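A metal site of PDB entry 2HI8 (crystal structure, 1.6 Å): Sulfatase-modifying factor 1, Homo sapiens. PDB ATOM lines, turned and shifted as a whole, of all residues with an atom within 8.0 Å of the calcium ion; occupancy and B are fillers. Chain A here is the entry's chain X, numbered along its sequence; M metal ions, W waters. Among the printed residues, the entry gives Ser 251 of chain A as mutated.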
ATOM      1  N   HIS A 171       2.464 -10.119 -22.440  1.00  0.00           N
ATOM      2  CA  HIS A 171       1.883 -10.241 -21.129  1.00  0.00           C
ATOM      3  C   HIS A 171       3.005 -10.482 -20.126  1.00  0.00           C
ATOM      4  O   HIS A 171       3.883 -11.333 -20.344  1.00  0.00           O
ATOM      5  CB  HIS A 171       0.823 -11.340 -21.098  1.00  0.00           C
ATOM      6  CG  HIS A 171      -0.479 -10.884 -21.682  1.00  0.00           C
ATOM      7  ND1 HIS A 171      -1.345 -10.065 -20.995  1.00  0.00           N
ATOM      8  CD2 HIS A 171      -1.007 -11.054 -22.909  1.00  0.00           C
ATOM      9  CE1 HIS A 171      -2.373  -9.767 -21.762  1.00  0.00           C
ATOM     10  NE2 HIS A 171      -2.193 -10.364 -22.937  1.00  0.00           N
ATOM     11  N   ALA A 173       2.152 -10.601 -16.563  1.00  0.00           N
ATOM     12  CA  ALA A 173       1.540 -11.141 -15.360  1.00  0.00           C
ATOM     13  C   ALA A 173       0.239 -11.828 -15.713  1.00  0.00           C
ATOM     14  O   ALA A 173      -0.404 -11.509 -16.738  1.00  0.00           O
ATOM     15  CB  ALA A 173       1.279 -10.026 -14.329  1.00  0.00           C
ATOM     16  N   ASN A 174      -0.147 -12.759 -14.863  1.00  0.00           N
ATOM     17  CA  ASN A 174      -1.389 -13.483 -15.031  1.00  0.00           C
ATOM     18  C   ASN A 174      -2.505 -12.764 -14.285  1.00  0.00           C
ATOM     19  O   ASN A 174      -2.622 -12.863 -13.071  1.00  0.00           O
ATOM     20  CB  ASN A 174      -1.234 -14.905 -14.539  1.00  0.00           C
ATOM     21  CG  ASN A 174      -2.499 -15.706 -14.646  1.00  0.00           C
ATOM     22  OD1 ASN A 174      -3.391 -15.366 -15.424  1.00  0.00           O
ATOM     23  ND2 ASN A 174      -2.590 -16.775 -13.856  1.00  0.00           N
ATOM     24  N   ILE A 175      -3.315 -12.008 -15.035  1.00  0.00           N
ATOM     25  CA  ILE A 175      -4.484 -11.327 -14.502  1.00  0.00           C
ATOM     26  C   ILE A 175      -5.670 -11.706 -15.404  1.00  0.00           C
ATOM     27  O   ILE A 175      -5.582 -12.661 -16.159  1.00  0.00           O
ATOM     28  CB  ILE A 175      -4.238  -9.812 -14.353  1.00  0.00           C
ATOM     29  CG1 ILE A 175      -3.941  -9.153 -15.699  1.00  0.00           C
ATOM     30  CG2 ILE A 175      -3.083  -9.570 -13.366  1.00  0.00           C
ATOM     31  CD1 ILE A 175      -3.865  -7.642 -15.610  1.00  0.00           C
ATOM     32  N   TRP A 176      -6.763 -10.951 -15.318  1.00  0.00           N
ATOM     33  CA  TRP A 176      -7.941 -11.216 -16.114  1.00  0.00           C
ATOM     34  C   TRP A 176      -7.892 -10.432 -17.407  1.00  0.00           C
ATOM     35  O   TRP A 176      -7.515  -9.255 -17.413  1.00  0.00           O
ATOM     36  CB  TRP A 176      -9.149 -10.804 -15.305  1.00  0.00           C
ATOM     37  CG  TRP A 176     -10.468 -11.126 -15.860  1.00  0.00           C
ATOM     38  CD1 TRP A 176     -11.162 -10.462 -16.839  1.00  0.00           C
ATOM     39  CD2 TRP A 176     -11.305 -12.175 -15.416  1.00  0.00           C
ATOM     40  NE1 TRP A 176     -12.396 -11.048 -17.024  1.00  0.00           N
ATOM     41  CE2 TRP A 176     -12.501 -12.112 -16.163  1.00  0.00           C
ATOM     42  CE3 TRP A 176     -11.164 -13.163 -14.445  1.00  0.00           C
ATOM     43  CZ2 TRP A 176     -13.549 -13.018 -15.962  1.00  0.00           C
ATOM     44  CZ3 TRP A 176     -12.204 -14.064 -14.242  1.00  0.00           C
ATOM     45  CH2 TRP A 176     -13.384 -13.982 -15.000  1.00  0.00           C
ATOM     46  N   GLN A 177      -8.268 -11.070 -18.507  1.00  0.00           N
ATOM     47  CA  GLN A 177      -8.599 -10.329 -19.701  1.00  0.00           C
ATOM     48  C   GLN A 177     -10.040 -10.630 -20.032  1.00  0.00           C
ATOM     49  O   GLN A 177     -10.471 -11.760 -19.910  1.00  0.00           O
ATOM     50  CB  GLN A 177      -7.715 -10.636 -20.898  1.00  0.00           C
ATOM     51  CG  GLN A 177      -6.301 -10.209 -20.716  1.00  0.00           C
ATOM     52  CD  GLN A 177      -5.531 -11.268 -19.992  1.00  0.00           C
ATOM     53  OE1 GLN A 177      -5.703 -12.448 -20.280  1.00  0.00           O
ATOM     54  NE2 GLN A 177      -4.657 -10.870 -19.061  1.00  0.00           N
ATOM     55  N   ASN A 184     -13.479 -14.515 -18.986  1.00  0.00           N
ATOM     56  CA  ASN A 184     -12.031 -14.441 -18.968  1.00  0.00           C
ATOM     57  C   ASN A 184     -11.529 -15.075 -20.251  1.00  0.00           C
ATOM     58  O   ASN A 184     -11.634 -16.290 -20.455  1.00  0.00           O
ATOM     59  CB  ASN A 184     -11.465 -15.164 -17.751  1.00  0.00           C
ATOM     60  CG  ASN A 184      -9.978 -14.943 -17.564  1.00  0.00           C
ATOM     61  OD1 ASN A 184      -9.296 -14.448 -18.451  1.00  0.00           O
ATOM     62  ND2 ASN A 184      -9.469 -15.315 -16.399  1.00  0.00           N
ATOM     63  N   THR A 185     -10.962 -14.253 -21.123  1.00  0.00           N
ATOM     64  CA  THR A 185     -10.549 -14.728 -22.424  1.00  0.00           C
ATOM     65  C   THR A 185      -9.321 -15.636 -22.386  1.00  0.00           C
ATOM     66  O   THR A 185      -9.048 -16.347 -23.339  1.00  0.00           O
ATOM     67  CB  THR A 185     -10.243 -13.558 -23.352  1.00  0.00           C
ATOM     68  OG1 THR A 185      -9.071 -12.881 -22.882  1.00  0.00           O
ATOM     69  CG2 THR A 185     -11.424 -12.577 -23.408  1.00  0.00           C
ATOM     70  N   GLY A 186      -8.560 -15.603 -21.288  1.00  0.00           N
ATOM     71  CA  GLY A 186      -7.322 -16.362 -21.182  1.00  0.00           C
ATOM     72  C   GLY A 186      -6.271 -15.920 -22.183  1.00  0.00           C
ATOM     73  O   GLY A 186      -5.383 -16.691 -22.540  1.00  0.00           O
ATOM     74  N   GLU A 187      -6.372 -14.677 -22.623  1.00  0.00           N
ATOM     75  CA  GLU A 187      -5.403 -14.090 -23.526  1.00  0.00           C
ATOM     76  C   GLU A 187      -3.970 -14.239 -23.050  1.00  0.00           C
ATOM     77  O   GLU A 187      -3.066 -14.485 -23.863  1.00  0.00           O
ATOM     78  CB  GLU A 187      -5.726 -12.615 -23.742  1.00  0.00           C
ATOM     79  CG  GLU A 187      -4.815 -11.924 -24.693  1.00  0.00           C
ATOM     80  CD  GLU A 187      -5.002 -10.435 -24.686  1.00  0.00           C
ATOM     81  OE1 GLU A 187      -6.116  -9.952 -24.371  1.00  0.00           O
ATOM     82  OE2 GLU A 187      -4.002  -9.754 -24.995  1.00  0.00           O
ATOM     83  N   ASP A 188      -3.734 -14.088 -21.745  1.00  0.00           N
ATOM     84  CA  ASP A 188      -2.360 -14.145 -21.220  1.00  0.00           C
ATOM     85  C   ASP A 188      -1.839 -15.582 -21.050  1.00  0.00           C
ATOM     86  O   ASP A 188      -0.709 -15.793 -20.609  1.00  0.00           O
ATOM     87  CB  ASP A 188      -2.245 -13.361 -19.921  1.00  0.00           C
ATOM     88  CG  ASP A 188      -3.081 -13.900 -18.810  1.00  0.00           C
ATOM     89  OD1 ASP A 188      -3.474 -15.101 -18.861  1.00  0.00           O
ATOM     90  OD2 ASP A 188      -3.381 -13.134 -17.874  1.00  0.00           O
ATOM     91  N   GLY A 189      -2.687 -16.551 -21.424  1.00  0.00           N
ATOM     92  CA  GLY A 189      -2.312 -17.957 -21.420  1.00  0.00           C
ATOM     93  C   GLY A 189      -2.848 -18.776 -20.274  1.00  0.00           C
ATOM     94  O   GLY A 189      -2.659 -19.988 -20.236  1.00  0.00           O
ATOM     95  N   PHE A 190      -3.533 -18.122 -19.321  1.00  0.00           N
ATOM     96  CA  PHE A 190      -4.023 -18.783 -18.125  1.00  0.00           C
ATOM     97  C   PHE A 190      -5.321 -18.177 -17.690  1.00  0.00           C
ATOM     98  O   PHE A 190      -5.388 -16.972 -17.459  1.00  0.00           O
ATOM     99  CB  PHE A 190      -2.991 -18.645 -17.013  1.00  0.00           C
ATOM    100  CG  PHE A 190      -1.680 -19.200 -17.398  1.00  0.00           C
ATOM    101  CD1 PHE A 190      -1.433 -20.556 -17.312  1.00  0.00           C
ATOM    102  CD2 PHE A 190      -0.703 -18.371 -17.946  1.00  0.00           C
ATOM    103  CE1 PHE A 190      -0.265 -21.101 -17.716  1.00  0.00           C
ATOM    104  CE2 PHE A 190       0.495 -18.913 -18.337  1.00  0.00           C
ATOM    105  CZ  PHE A 190       0.711 -20.291 -18.229  1.00  0.00           C
ATOM    106  N   GLN A 191      -6.341 -19.004 -17.571  1.00  0.00           N
ATOM    107  CA  GLN A 191      -7.610 -18.529 -17.024  1.00  0.00           C
ATOM    108  C   GLN A 191      -7.566 -18.554 -15.509  1.00  0.00           C
ATOM    109  O   GLN A 191      -7.905 -17.566 -14.897  1.00  0.00           O
ATOM    110  CB  GLN A 191      -8.786 -19.302 -17.603  1.00  0.00           C
ATOM    111  CG  GLN A 191      -9.009 -18.927 -19.059  1.00  0.00           C
ATOM    112  CD  GLN A 191     -10.017 -19.797 -19.755  1.00  0.00           C
ATOM    113  OE1 GLN A 191      -9.962 -21.025 -19.647  1.00  0.00           O
ATOM    114  NE2 GLN A 191     -10.944 -19.185 -20.479  1.00  0.00           N
ATOM    115  N   GLY A 192      -7.120 -19.667 -14.918  1.00  0.00           N
ATOM    116  CA  GLY A 192      -6.898 -19.735 -13.503  1.00  0.00           C
ATOM    117  C   GLY A 192      -5.450 -19.394 -13.265  1.00  0.00           C
ATOM    118  O   GLY A 192      -4.872 -18.559 -13.938  1.00  0.00           O
ATOM    119  N   THR A 193      -4.845 -20.068 -12.293  1.00  0.00           N
ATOM    120  CA  THR A 193      -3.457 -19.813 -11.977  1.00  0.00           C
ATOM    121  C   THR A 193      -2.532 -20.293 -13.095  1.00  0.00           C
ATOM    122  O   THR A 193      -2.912 -21.097 -13.989  1.00  0.00           O
ATOM    123  CB  THR A 193      -3.054 -20.528 -10.677  1.00  0.00           C
ATOM    124  OG1 THR A 193      -3.365 -21.919 -10.817  1.00  0.00           O
ATOM    125  CG2 THR A 193      -3.805 -19.959  -9.476  1.00  0.00           C
ATOM    126  N   ALA A 194      -1.308 -19.777 -13.049  1.00  0.00           N
ATOM    127  CA  ALA A 194      -0.233 -20.227 -13.901  1.00  0.00           C
ATOM    128  C   ALA A 194       0.825 -20.863 -13.018  1.00  0.00           C
ATOM    129  O   ALA A 194       0.879 -20.595 -11.811  1.00  0.00           O
ATOM    130  CB  ALA A 194       0.379 -19.059 -14.691  1.00  0.00           C
ATOM    131  N   PHE A 199       5.838 -16.287 -16.650  1.00  0.00           N
ATOM    132  CA  PHE A 199       5.984 -14.856 -16.931  1.00  0.00           C
ATOM    133  C   PHE A 199       7.383 -14.378 -16.609  1.00  0.00           C
ATOM    134  O   PHE A 199       8.141 -15.091 -15.963  1.00  0.00           O
ATOM    135  CB  PHE A 199       4.868 -14.053 -16.266  1.00  0.00           C
ATOM    136  CG  PHE A 199       3.524 -14.389 -16.829  1.00  0.00           C
ATOM    137  CD1 PHE A 199       3.158 -13.900 -18.089  1.00  0.00           C
ATOM    138  CD2 PHE A 199       2.691 -15.270 -16.182  1.00  0.00           C
ATOM    139  CE1 PHE A 199       1.958 -14.236 -18.651  1.00  0.00           C
ATOM    140  CE2 PHE A 199       1.474 -15.621 -16.741  1.00  0.00           C
ATOM    141  CZ  PHE A 199       1.119 -15.118 -17.983  1.00  0.00           C
ATOM    142  N   ASN A 212      -1.509 -13.735 -10.615  1.00  0.00           N
ATOM    143  CA  ASN A 212      -1.489 -15.150 -10.279  1.00  0.00           C
ATOM    144  C   ASN A 212      -2.212 -15.380  -8.969  1.00  0.00           C
ATOM    145  O   ASN A 212      -3.432 -15.364  -8.959  1.00  0.00           O
ATOM    146  CB  ASN A 212      -0.073 -15.750 -10.347  1.00  0.00           C
ATOM    147  CG  ASN A 212      -0.069 -17.164 -10.894  1.00  0.00           C
ATOM    148  OD1 ASN A 212      -0.892 -17.517 -11.733  1.00  0.00           O
ATOM    149  ND2 ASN A 212       0.864 -17.986 -10.439  1.00  0.00           N
ATOM    150  N   SER A 248      -4.229 -10.919  -8.431  1.00  0.00           N
ATOM    151  CA  SER A 248      -4.349 -12.302  -8.803  1.00  0.00           C
ATOM    152  C   SER A 248      -4.779 -12.427 -10.231  1.00  0.00           C
ATOM    153  O   SER A 248      -4.991 -11.439 -10.943  1.00  0.00           O
ATOM    154  CB  SER A 248      -5.385 -13.015  -7.911  1.00  0.00           C
ATOM    155  OG  SER A 248      -6.711 -12.743  -8.310  1.00  0.00           O
ATOM    156  N   TYR A 249      -4.913 -13.669 -10.631  1.00  0.00           N
ATOM    157  CA  TYR A 249      -5.437 -14.027 -11.935  1.00  0.00           C
ATOM    158  C   TYR A 249      -6.839 -13.512 -12.206  1.00  0.00           C
ATOM    159  O   TYR A 249      -7.280 -13.508 -13.351  1.00  0.00           O
ATOM    160  CB  TYR A 249      -5.348 -15.542 -12.115  1.00  0.00           C
ATOM    161  CG  TYR A 249      -6.341 -16.376 -11.321  1.00  0.00           C
ATOM    162  CD1 TYR A 249      -7.628 -16.529 -11.763  1.00  0.00           C
ATOM    163  CD2 TYR A 249      -5.945 -17.062 -10.164  1.00  0.00           C
ATOM    164  CE1 TYR A 249      -8.540 -17.306 -11.063  1.00  0.00           C
ATOM    165  CE2 TYR A 249      -6.851 -17.851  -9.459  1.00  0.00           C
ATOM    166  CZ  TYR A 249      -8.139 -17.958  -9.911  1.00  0.00           C
ATOM    167  OH  TYR A 249      -9.056 -18.751  -9.241  1.00  0.00           O
ATOM    168  N   MET A 250      -7.536 -13.051 -11.163  1.00  0.00           N
ATOM    169  CA  MET A 250      -8.862 -12.443 -11.316  1.00  0.00           C
ATOM    170  C   MET A 250      -8.834 -10.927 -11.462  1.00  0.00           C
ATOM    171  O   MET A 250      -9.873 -10.293 -11.769  1.00  0.00           O
ATOM    172  CB  MET A 250      -9.722 -12.794 -10.105  1.00  0.00           C
ATOM    173  CG  MET A 250     -10.093 -14.236 -10.002  1.00  0.00           C
ATOM    174  SD  MET A 250     -10.815 -14.576  -8.377  1.00  0.00           S
ATOM    175  CE  MET A 250     -12.326 -13.607  -8.476  1.00  0.00           C
ATOM    176  N   SER A 251      -7.687 -10.321 -11.233  1.00  0.00           N
ATOM    177  CA  SER A 251      -7.580  -8.879 -11.226  1.00  0.00           C
ATOM    178  C   SER A 251      -7.765  -8.282 -12.609  1.00  0.00           C
ATOM    179  O   SER A 251      -7.357  -8.837 -13.635  1.00  0.00           O
ATOM    180  CB  SER A 251      -6.256  -8.428 -10.625  1.00  0.00           C
ATOM    181  OG  SER A 251      -6.084  -8.944  -9.312  1.00  0.00           O
HETATM  182 CA    CA M   1      -4.978 -14.773 -16.945  1.00  0.00          CA
HETATM  183  O   HOH W   1      -6.629 -14.350 -18.625  1.00  0.00           O
HETATM  184  O   HOH W   2      -6.715 -15.131 -15.361  1.00  0.00           O
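The backbone carbonyl oxygen of Asn 174 lies close to the backbone NH of Tyr 249, 3.4 Å away.
O of Gly 192 is in hydrogen-bond range of ND2 of Asn 174, at 2.9 Å.
The side-chain amide nitrogen (ND2) of Asn 174 lies within hydrogen-bond range of the side-chain amide oxygen (OD1) of Asn 212.
The side-chain amide nitrogen (ND2) of Asn 174 lies close to the backbone NH (N) of Ala 194 (3.4 Å).
The side-chain amide oxygen of Gln 177 is in hydrogen-bond range of the backbone NH of Asp 188, 3.0 Å away.
Of the 23 residues printed, 4 come within 4 Å of the calcium ion.
Water W2 lies within hydrogen-bond range of O of Tyr 249 (2.6 Å), O of Gln 191 (2.7 Å) and ND2 of Asn 184 (2.9 Å).
Water W1 lies within hydrogen-bond range of the side-chain amide oxygen of Asn 184 and the side-chain amide oxygen of Gln 177.
The calcium ion is bound by OD1 of Asn 174 (2.3 Å).
The calcium ion is bound by the backbone carbonyl oxygen (O) of Phe 190, at 2.3 Å.
The calcium ion is bound by the backbone carbonyl oxygen (O) of Ile 175 (2.3 Å).
Water W2 binds the calcium ion (2.4 Å).
The calcium ion is bound by water W1, at 2.4 Å.
The side-chain carboxylate (OD1) of Asp 188 binds the calcium ion.
OD2 of Asp 188 is bound to the calcium ion (2.5 Å).
The calcium ion has seven donor atoms within binding distance.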
